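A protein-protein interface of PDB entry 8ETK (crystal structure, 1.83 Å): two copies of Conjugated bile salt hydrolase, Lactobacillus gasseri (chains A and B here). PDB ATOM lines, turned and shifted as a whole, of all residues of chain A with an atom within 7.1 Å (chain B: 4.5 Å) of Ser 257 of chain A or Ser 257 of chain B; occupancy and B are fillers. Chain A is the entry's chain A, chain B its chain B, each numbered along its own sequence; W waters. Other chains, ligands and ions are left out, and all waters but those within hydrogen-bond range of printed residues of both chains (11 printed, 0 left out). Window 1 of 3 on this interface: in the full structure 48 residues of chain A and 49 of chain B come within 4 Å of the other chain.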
ATOM      1  N   ASN A  19      -5.686  -5.634 -26.249  1.00  0.00           N
ATOM      2  CA  ASN A  19      -5.297  -7.036 -26.055  1.00  0.00           C
ATOM      3  C   ASN A  19      -6.552  -7.904 -26.056  1.00  0.00           C
ATOM      4  O   ASN A  19      -7.576  -7.529 -25.475  1.00  0.00           O
ATOM      5  CB  ASN A  19      -4.606  -7.263 -24.702  1.00  0.00           C
ATOM      6  CG  ASN A  19      -3.203  -6.688 -24.628  1.00  0.00           C
ATOM      7  OD1 ASN A  19      -2.534  -6.504 -25.639  1.00  0.00           O
ATOM      8  ND2 ASN A  19      -2.748  -6.419 -23.407  1.00  0.00           N
ATOM      9  N   GLY A 220       0.678  -6.139 -10.301  1.00  0.00           N
ATOM     10  CA  GLY A 220       1.166  -6.748 -11.521  1.00  0.00           C
ATOM     11  C   GLY A 220       0.424  -7.999 -11.945  1.00  0.00           C
ATOM     12  O   GLY A 220       0.817  -8.646 -12.913  1.00  0.00           O
ATOM     13  N   LYS A 230      -3.073  -0.274 -13.482  1.00  0.00           N
ATOM     14  CA  LYS A 230      -1.735  -0.160 -14.056  1.00  0.00           C
ATOM     15  C   LYS A 230      -1.775   0.469 -15.445  1.00  0.00           C
ATOM     16  O   LYS A 230      -0.938   1.322 -15.767  1.00  0.00           O
ATOM     17  CB  LYS A 230      -1.037  -1.521 -14.116  1.00  0.00           C
ATOM     18  CG  LYS A 230       0.402  -1.413 -14.680  1.00  0.00           C
ATOM     19  CD  LYS A 230       1.217  -2.695 -14.503  1.00  0.00           C
ATOM     20  CE  LYS A 230       2.587  -2.560 -15.186  1.00  0.00           C
ATOM     21  NZ  LYS A 230       3.504  -3.699 -14.914  1.00  0.00           N
ATOM     22  N   LEU A 234       0.063   3.871 -16.457  1.00  0.00           N
ATOM     23  CA  LEU A 234       1.052   3.924 -17.535  1.00  0.00           C
ATOM     24  C   LEU A 234       0.636   4.900 -18.629  1.00  0.00           C
ATOM     25  O   LEU A 234       1.464   5.683 -19.115  1.00  0.00           O
ATOM     26  CB  LEU A 234       1.283   2.539 -18.140  1.00  0.00           C
ATOM     27  CG  LEU A 234       1.909   1.492 -17.232  1.00  0.00           C
ATOM     28  CD1 LEU A 234       2.126   0.207 -18.006  1.00  0.00           C
ATOM     29  CD2 LEU A 234       3.217   1.995 -16.627  1.00  0.00           C
ATOM     30  N   PHE A 251       2.458   2.182 -28.034  1.00  0.00           N
ATOM     31  CA  PHE A 251       1.216   1.448 -27.816  1.00  0.00           C
ATOM     32  C   PHE A 251       1.490   0.015 -27.368  1.00  0.00           C
ATOM     33  O   PHE A 251       0.931  -0.455 -26.365  1.00  0.00           O
ATOM     34  CB  PHE A 251       0.386   1.467 -29.105  1.00  0.00           C
ATOM     35  CG  PHE A 251      -0.963   0.830 -28.958  1.00  0.00           C
ATOM     36  CD1 PHE A 251      -1.105  -0.543 -29.072  1.00  0.00           C
ATOM     37  CD2 PHE A 251      -2.082   1.609 -28.688  1.00  0.00           C
ATOM     38  CE1 PHE A 251      -2.349  -1.133 -28.921  1.00  0.00           C
ATOM     39  CE2 PHE A 251      -3.331   1.031 -28.535  1.00  0.00           C
ATOM     40  CZ  PHE A 251      -3.466  -0.333 -28.636  1.00  0.00           C
ATOM     41  N   PHE A 252       2.334  -0.704 -28.114  1.00  0.00           N
ATOM     42  CA  PHE A 252       2.634  -2.089 -27.764  1.00  0.00           C
ATOM     43  C   PHE A 252       3.432  -2.179 -26.471  1.00  0.00           C
ATOM     44  O   PHE A 252       3.291  -3.158 -25.733  1.00  0.00           O
ATOM     45  CB  PHE A 252       3.373  -2.782 -28.920  1.00  0.00           C
ATOM     46  CG  PHE A 252       2.448  -3.273 -30.016  1.00  0.00           C
ATOM     47  CD1 PHE A 252       1.971  -2.388 -30.989  1.00  0.00           C
ATOM     48  CD2 PHE A 252       2.047  -4.601 -30.075  1.00  0.00           C
ATOM     49  CE1 PHE A 252       1.106  -2.815 -31.988  1.00  0.00           C
ATOM     50  CE2 PHE A 252       1.168  -5.041 -31.078  1.00  0.00           C
ATOM     51  CZ  PHE A 252       0.699  -4.148 -32.028  1.00  0.00           C
ATOM     52  N   ASN A 253       4.264  -1.174 -26.166  1.00  0.00           N
ATOM     53  CA  ASN A 253       4.968  -1.177 -24.885  1.00  0.00           C
ATOM     54  C   ASN A 253       3.976  -1.229 -23.726  1.00  0.00           C
ATOM     55  O   ASN A 253       4.125  -2.028 -22.793  1.00  0.00           O
ATOM     56  CB  ASN A 253       5.848   0.071 -24.755  1.00  0.00           C
ATOM     57  CG  ASN A 253       7.028   0.082 -25.724  1.00  0.00           C
ATOM     58  OD1 ASN A 253       7.524  -0.956 -26.156  1.00  0.00           O
ATOM     59  ND2 ASN A 253       7.476   1.277 -26.062  1.00  0.00           N
ATOM     60  N   ILE A 254       2.954  -0.378 -23.777  1.00  0.00           N
ATOM     61  CA  ILE A 254       1.966  -0.315 -22.704  1.00  0.00           C
ATOM     62  C   ILE A 254       1.148  -1.601 -22.649  1.00  0.00           C
ATOM     63  O   ILE A 254       1.008  -2.213 -21.589  1.00  0.00           O
ATOM     64  CB  ILE A 254       1.056   0.916 -22.875  1.00  0.00           C
ATOM     65  CG1 ILE A 254       1.849   2.218 -22.693  1.00  0.00           C
ATOM     66  CG2 ILE A 254      -0.133   0.837 -21.891  1.00  0.00           C
ATOM     67  CD1 ILE A 254       1.074   3.490 -23.142  1.00  0.00           C
ATOM     68  N   LEU A 255       0.595  -2.036 -23.787  1.00  0.00           N
ATOM     69  CA  LEU A 255      -0.276  -3.207 -23.734  1.00  0.00           C
ATOM     70  C   LEU A 255       0.513  -4.496 -23.477  1.00  0.00           C
ATOM     71  O   LEU A 255      -0.019  -5.416 -22.855  1.00  0.00           O
ATOM     72  CB  LEU A 255      -1.122  -3.315 -25.011  1.00  0.00           C
ATOM     73  CG  LEU A 255      -2.391  -2.443 -25.013  1.00  0.00           C
ATOM     74  CD1 LEU A 255      -3.389  -2.861 -26.121  1.00  0.00           C
ATOM     75  CD2 LEU A 255      -3.112  -2.475 -23.665  1.00  0.00           C
ATOM     76  N   LYS A 256       1.780  -4.594 -23.912  1.00  0.00           N
ATOM     77  CA  LYS A 256       2.532  -5.784 -23.533  1.00  0.00           C
ATOM     78  C   LYS A 256       2.885  -5.776 -22.047  1.00  0.00           C
ATOM     79  O   LYS A 256       3.060  -6.848 -21.453  1.00  0.00           O
ATOM     80  CB  LYS A 256       3.798  -5.940 -24.388  1.00  0.00           C
ATOM     81  CG  LYS A 256       3.481  -6.305 -25.833  1.00  0.00           C
ATOM     82  CD  LYS A 256       2.500  -7.497 -25.922  1.00  0.00           C
ATOM     83  CE  LYS A 256       2.459  -8.056 -27.352  1.00  0.00           C
ATOM     84  NZ  LYS A 256       1.420  -9.134 -27.527  1.00  0.00           N
ATOM     85  N   SER A 257       2.948  -4.594 -21.433  1.00  0.00           N
ATOM     86  CA  SER A 257       3.219  -4.516 -19.999  1.00  0.00           C
ATOM     87  C   SER A 257       2.070  -5.110 -19.174  1.00  0.00           C
ATOM     88  O   SER A 257       2.310  -5.712 -18.117  1.00  0.00           O
ATOM     89  CB  SER A 257       3.473  -3.059 -19.600  1.00  0.00           C
ATOM     90  OG  SER A 257       3.636  -2.934 -18.198  1.00  0.00           O
ATOM     91  N   VAL A 258       0.826  -4.936 -19.626  1.00  0.00           N
ATOM     92  CA  VAL A 258      -0.354  -5.432 -18.904  1.00  0.00           C
ATOM     93  C   VAL A 258      -0.944  -6.689 -19.557  1.00  0.00           C
ATOM     94  O   VAL A 258      -2.081  -7.068 -19.260  1.00  0.00           O
ATOM     95  CB  VAL A 258      -1.433  -4.343 -18.742  1.00  0.00           C
ATOM     96  CG1 VAL A 258      -0.920  -3.169 -17.904  1.00  0.00           C
ATOM     97  CG2 VAL A 258      -1.990  -3.884 -20.089  1.00  0.00           C
ATOM     98  N   ALA A 259      -0.206  -7.325 -20.457  1.00  0.00           N
ATOM     99  CA  ALA A 259      -0.674  -8.557 -21.074  1.00  0.00           C
ATOM    100  C   ALA A 259      -0.816  -9.684 -20.048  1.00  0.00           C
ATOM    101  O   ALA A 259      -0.103  -9.747 -19.044  1.00  0.00           O
ATOM    102  CB  ALA A 259       0.300  -8.988 -22.172  1.00  0.00           C
ATOM    103  N   MET A 260      -1.729 -10.609 -20.338  1.00  0.00           N
ATOM    104  CA  MET A 260      -1.917 -11.816 -19.542  1.00  0.00           C
ATOM    105  C   MET A 260      -0.986 -12.892 -20.095  1.00  0.00           C
ATOM    106  O   MET A 260      -1.164 -13.347 -21.230  1.00  0.00           O
ATOM    107  CB  MET A 260      -3.389 -12.226 -19.622  1.00  0.00           C
ATOM    108  CG  MET A 260      -3.846 -13.264 -18.650  1.00  0.00           C
ATOM    109  SD  MET A 260      -5.670 -13.428 -18.684  1.00  0.00           S
ATOM    110  CE  MET A 260      -6.268 -11.773 -18.400  1.00  0.00           C
ATOM    111  N   ILE A 261       0.016 -13.304 -19.300  1.00  0.00           N
ATOM    112  CA  ILE A 261       1.119 -14.121 -19.807  1.00  0.00           C
ATOM    113  C   ILE A 261       0.773 -15.597 -19.690  1.00  0.00           C
ATOM    114  O   ILE A 261       0.301 -16.064 -18.640  1.00  0.00           O
ATOM    115  CB  ILE A 261       2.420 -13.795 -19.052  1.00  0.00           C
ATOM    116  CG1 ILE A 261       2.705 -12.292 -19.157  1.00  0.00           C
ATOM    117  CG2 ILE A 261       3.615 -14.656 -19.570  1.00  0.00           C
ATOM    118  CD1 ILE A 261       2.618 -11.742 -20.593  1.00  0.00           C
ATOM    119  N   LYS B 230       8.400 -11.383 -10.303  1.00  0.00           N
ATOM    120  CA  LYS B 230       7.474 -11.577 -11.409  1.00  0.00           C
ATOM    121  C   LYS B 230       8.138 -12.297 -12.570  1.00  0.00           C
ATOM    122  O   LYS B 230       7.535 -13.193 -13.170  1.00  0.00           O
ATOM    123  CB  LYS B 230       6.893 -10.236 -11.862  1.00  0.00           C
ATOM    124  CG  LYS B 230       5.909 -10.392 -13.024  1.00  0.00           C
ATOM    125  CD  LYS B 230       5.059  -9.127 -13.267  1.00  0.00           C
ATOM    126  CE  LYS B 230       4.195  -9.330 -14.516  1.00  0.00           C
ATOM    127  NZ  LYS B 230       3.197  -8.238 -14.737  1.00  0.00           N
ATOM    128  N   LEU B 234       6.766 -15.871 -13.964  1.00  0.00           N
ATOM    129  CA  LEU B 234       6.353 -16.076 -15.350  1.00  0.00           C
ATOM    130  C   LEU B 234       7.188 -17.161 -16.027  1.00  0.00           C
ATOM    131  O   LEU B 234       6.644 -18.038 -16.709  1.00  0.00           O
ATOM    132  CB  LEU B 234       6.444 -14.759 -16.122  1.00  0.00           C
ATOM    133  CG  LEU B 234       5.515 -13.612 -15.668  1.00  0.00           C
ATOM    134  CD1 LEU B 234       5.698 -12.387 -16.562  1.00  0.00           C
ATOM    135  CD2 LEU B 234       4.016 -14.001 -15.606  1.00  0.00           C
ATOM    136  N   ASN B 253       7.404 -11.929 -24.929  1.00  0.00           N
ATOM    137  CA  ASN B 253       6.195 -11.816 -24.099  1.00  0.00           C
ATOM    138  C   ASN B 253       6.572 -11.617 -22.637  1.00  0.00           C
ATOM    139  O   ASN B 253       6.058 -10.715 -21.967  1.00  0.00           O
ATOM    140  CB  ASN B 253       5.322 -13.069 -24.246  1.00  0.00           C
ATOM    141  CG  ASN B 253       4.657 -13.178 -25.604  1.00  0.00           C
ATOM    142  OD1 ASN B 253       4.441 -12.181 -26.289  1.00  0.00           O
ATOM    143  ND2 ASN B 253       4.309 -14.408 -25.994  1.00  0.00           N
ATOM    144  N   ILE B 254       7.508 -12.438 -22.140  1.00  0.00           N
ATOM    145  CA  ILE B 254       7.924 -12.363 -20.741  1.00  0.00           C
ATOM    146  C   ILE B 254       8.654 -11.056 -20.463  1.00  0.00           C
ATOM    147  O   ILE B 254       8.322 -10.335 -19.519  1.00  0.00           O
ATOM    148  CB  ILE B 254       8.794 -13.579 -20.364  1.00  0.00           C
ATOM    149  CG1 ILE B 254       7.979 -14.876 -20.451  1.00  0.00           C
ATOM    150  CG2 ILE B 254       9.362 -13.412 -18.936  1.00  0.00           C
ATOM    151  CD1 ILE B 254       8.818 -16.145 -20.195  1.00  0.00           C
ATOM    152  N   LEU B 255       9.682 -10.732 -21.257  1.00  0.00           N
ATOM    153  CA  LEU B 255      10.452  -9.532 -20.936  1.00  0.00           C
ATOM    154  C   LEU B 255       9.650  -8.249 -21.153  1.00  0.00           C
ATOM    155  O   LEU B 255       9.843  -7.277 -20.416  1.00  0.00           O
ATOM    156  CB  LEU B 255      11.769  -9.506 -21.728  1.00  0.00           C
ATOM    157  CG  LEU B 255      12.882 -10.348 -21.080  1.00  0.00           C
ATOM    158  CD1 LEU B 255      14.248 -10.021 -21.674  1.00  0.00           C
ATOM    159  CD2 LEU B 255      12.955 -10.188 -19.561  1.00  0.00           C
ATOM    160  N   LYS B 256       8.721  -8.210 -22.116  1.00  0.00           N
ATOM    161  CA  LYS B 256       7.922  -6.993 -22.215  1.00  0.00           C
ATOM    162  C   LYS B 256       6.940  -6.871 -21.048  1.00  0.00           C
ATOM    163  O   LYS B 256       6.517  -5.758 -20.713  1.00  0.00           O
ATOM    164  CB  LYS B 256       7.166  -6.949 -23.547  1.00  0.00           C
ATOM    165  CG  LYS B 256       8.094  -6.800 -24.769  1.00  0.00           C
ATOM    166  CD  LYS B 256       9.007  -5.586 -24.584  1.00  0.00           C
ATOM    167  CE  LYS B 256       9.704  -5.245 -25.900  1.00  0.00           C
ATOM    168  NZ  LYS B 256      10.672  -4.138 -25.710  1.00  0.00           N
ATOM    169  N   SER B 257       6.588  -7.992 -20.414  1.00  0.00           N
ATOM    170  CA  SER B 257       5.705  -7.938 -19.249  1.00  0.00           C
ATOM    171  C   SER B 257       6.377  -7.246 -18.066  1.00  0.00           C
ATOM    172  O   SER B 257       5.705  -6.552 -17.288  1.00  0.00           O
ATOM    173  CB  SER B 257       5.263  -9.357 -18.864  1.00  0.00           C
ATOM    174  OG  SER B 257       4.486  -9.332 -17.675  1.00  0.00           O
ATOM    175  N   VAL B 258       7.693  -7.405 -17.916  1.00  0.00           N
ATOM    176  CA  VAL B 258       8.436  -6.809 -16.813  1.00  0.00           C
ATOM    177  C   VAL B 258       9.269  -5.614 -17.280  1.00  0.00           C
ATOM    178  O   VAL B 258      10.194  -5.197 -16.588  1.00  0.00           O
ATOM    179  CB  VAL B 258       9.318  -7.847 -16.097  1.00  0.00           C
ATOM    180  CG1 VAL B 258       8.458  -8.927 -15.469  1.00  0.00           C
ATOM    181  CG2 VAL B 258      10.359  -8.474 -17.080  1.00  0.00           C
ATOM    182  N   ALA B 259       8.960  -5.066 -18.448  1.00  0.00           N
ATOM    183  CA  ALA B 259       9.672  -3.893 -18.925  1.00  0.00           C
ATOM    184  C   ALA B 259       9.391  -2.691 -18.035  1.00  0.00           C
ATOM    185  O   ALA B 259       8.332  -2.574 -17.409  1.00  0.00           O
ATOM    186  CB  ALA B 259       9.272  -3.565 -20.364  1.00  0.00           C
ATOM    187  N   ILE B 261       8.518   1.015 -18.018  1.00  0.00           N
ATOM    188  CA  ILE B 261       7.742   1.727 -19.024  1.00  0.00           C
ATOM    189  C   ILE B 261       8.044   3.224 -18.948  1.00  0.00           C
ATOM    190  O   ILE B 261       8.015   3.821 -17.866  1.00  0.00           O
ATOM    191  CB  ILE B 261       6.246   1.444 -18.839  1.00  0.00           C
ATOM    192  CG1 ILE B 261       5.988  -0.066 -18.988  1.00  0.00           C
ATOM    193  CG2 ILE B 261       5.437   2.194 -19.888  1.00  0.00           C
ATOM    194  CD1 ILE B 261       6.463  -0.648 -20.337  1.00  0.00           C
HETATM  195  O   HOH W   1       8.621  -2.185 -23.894  1.00  0.00           O
HETATM  196  O   HOH W   2       5.032  -5.966 -14.694  1.00  0.00           O
HETATM  197  O   HOH W   3       0.675 -10.518 -15.031  1.00  0.00           O
HETATM  198  O   HOH W   4       2.724 -11.521 -28.362  1.00  0.00           O
HETATM  199  O   HOH W   5       3.877  -9.280 -22.868  1.00  0.00           O
HETATM  200  O   HOH W   6       5.966  -3.769 -17.090  1.00  0.00           O
HETATM  201  O   HOH W   7       1.913  -8.450 -17.636  1.00  0.00           O
HETATM  202  O   HOH W   8       1.886  -5.867 -15.435  1.00  0.00           O
HETATM  203  O   HOH W   9       6.489  -3.518 -22.659  1.00  0.00           O
HETATM  204  O   HOH W  10       9.961  -1.774 -27.231  1.00  0.00           O
HETATM  205  O   HOH W  11       2.361 -10.712 -24.918  1.00  0.00           O
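The side-chain hydroxyl of Ser 257 of chain A lies close to the side-chain amino group of Lys 230 of chain A. NZ of Lys 230 of chain B lies close to OG of Ser 257 of chain B, at 3.4 Å.
O of Gly 220 of chain A is in hydrogen-bond range of NZ of Lys 230 of chain B, 3.0 Å away.
Printed residues of chain B that touch a printed residue of chain A: Lys 230, Leu 234, Asn 253, Lys 256, Ser 257 and Ile 261. Hydrophobic or aromatic side chains of chain A within 4 Å of the printed part of chain B: Leu 234 and Ile 261.
Leu 234 of chain A touches Ile 261 of chain B, and with the chains exchanged Ile 261 of chain A touches Leu 234 of chain B. Lys 256 of chain B touches its own counterpart, Lys 256 of chain A. Ser 257 of chain A touches its own counterpart, Ser 257 of chain B. Ser 257 of chain A touches Ile 261 of chain B, and with the chains exchanged Ile 261 of chain A touches Ser 257 of chain B. Of the 11 pairs that touch across the chains among the printed residues, 10 have their exchanged pair printed and touching as well.
Water W8 lies within hydrogen-bond range of O of Ser 257 of chain A (2.7 Å), NZ of Lys 230 of chain A (2.8 Å) and NZ of Lys 230 of chain B (2.8 Å). Water W5 lies within hydrogen-bond range of O of Asn 253 of chain B (2.8 Å) and O of Lys 256 of chain A (2.9 Å). Water W4 lies within hydrogen-bond range of OD1 of Asn 253 of chain B and NZ of Lys 256 of chain A. Water W10 bridges OD1 of Asn 253 of chain A and NZ of Lys 256 of chain B. Water W3 lies within hydrogen-bond range of the backbone carbonyl oxygen of Gly 220 of chain A (2.8 Å) and the side-chain amino group of Lys 230 of chain B (3.4 Å). Water W11 bridges OD1 of Asn 253 of chain B and NZ of Lys 256 of chain A.
Of the printed residues of chain B, Leu 234 of chain A touches Ile 261. Leu 255 of chain A touches none of the printed residues of chain B. Of chain B, only Lys 256 (3.6 Å), Ser 257 (3.6 Å) and Ile 261 (3.8 Å) come within 4 Å of Ser 257 of chain A. Of the printed residues of chain A, Asn 253 of chain B touches Ile 261. The nearest residue of chain A that does not touch Ser 257 of chain B is Lys 230 of chain A (4.3 Å).
Among the printed residues, pairs that only touch across the chains: Leu 234 of chain A with Ile 261 of chain B (3.8 Å), Asn 253 of chain A with Ile 261 of chain B (3.7 Å), Lys 256 of chain A with Lys 256 of chain B (3.6 Å), Lys 256 of chain A with Ser 257 of chain B (3.6 Å), Ser 257 of chain A with Lys 256 of chain B (3.6 Å), Ser 257 of chain A with Ser 257 of chain B (3.6 Å), Ser 257 of chain A with Ile 261 of chain B (3.8 Å), Ile 261 of chain A with Leu 234 of chain B (3.8 Å), Ile 261 of chain A with Asn 253 of chain B (3.8 Å) and Ile 261 of chain A with Ser 257 of chain B (3.8 Å).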
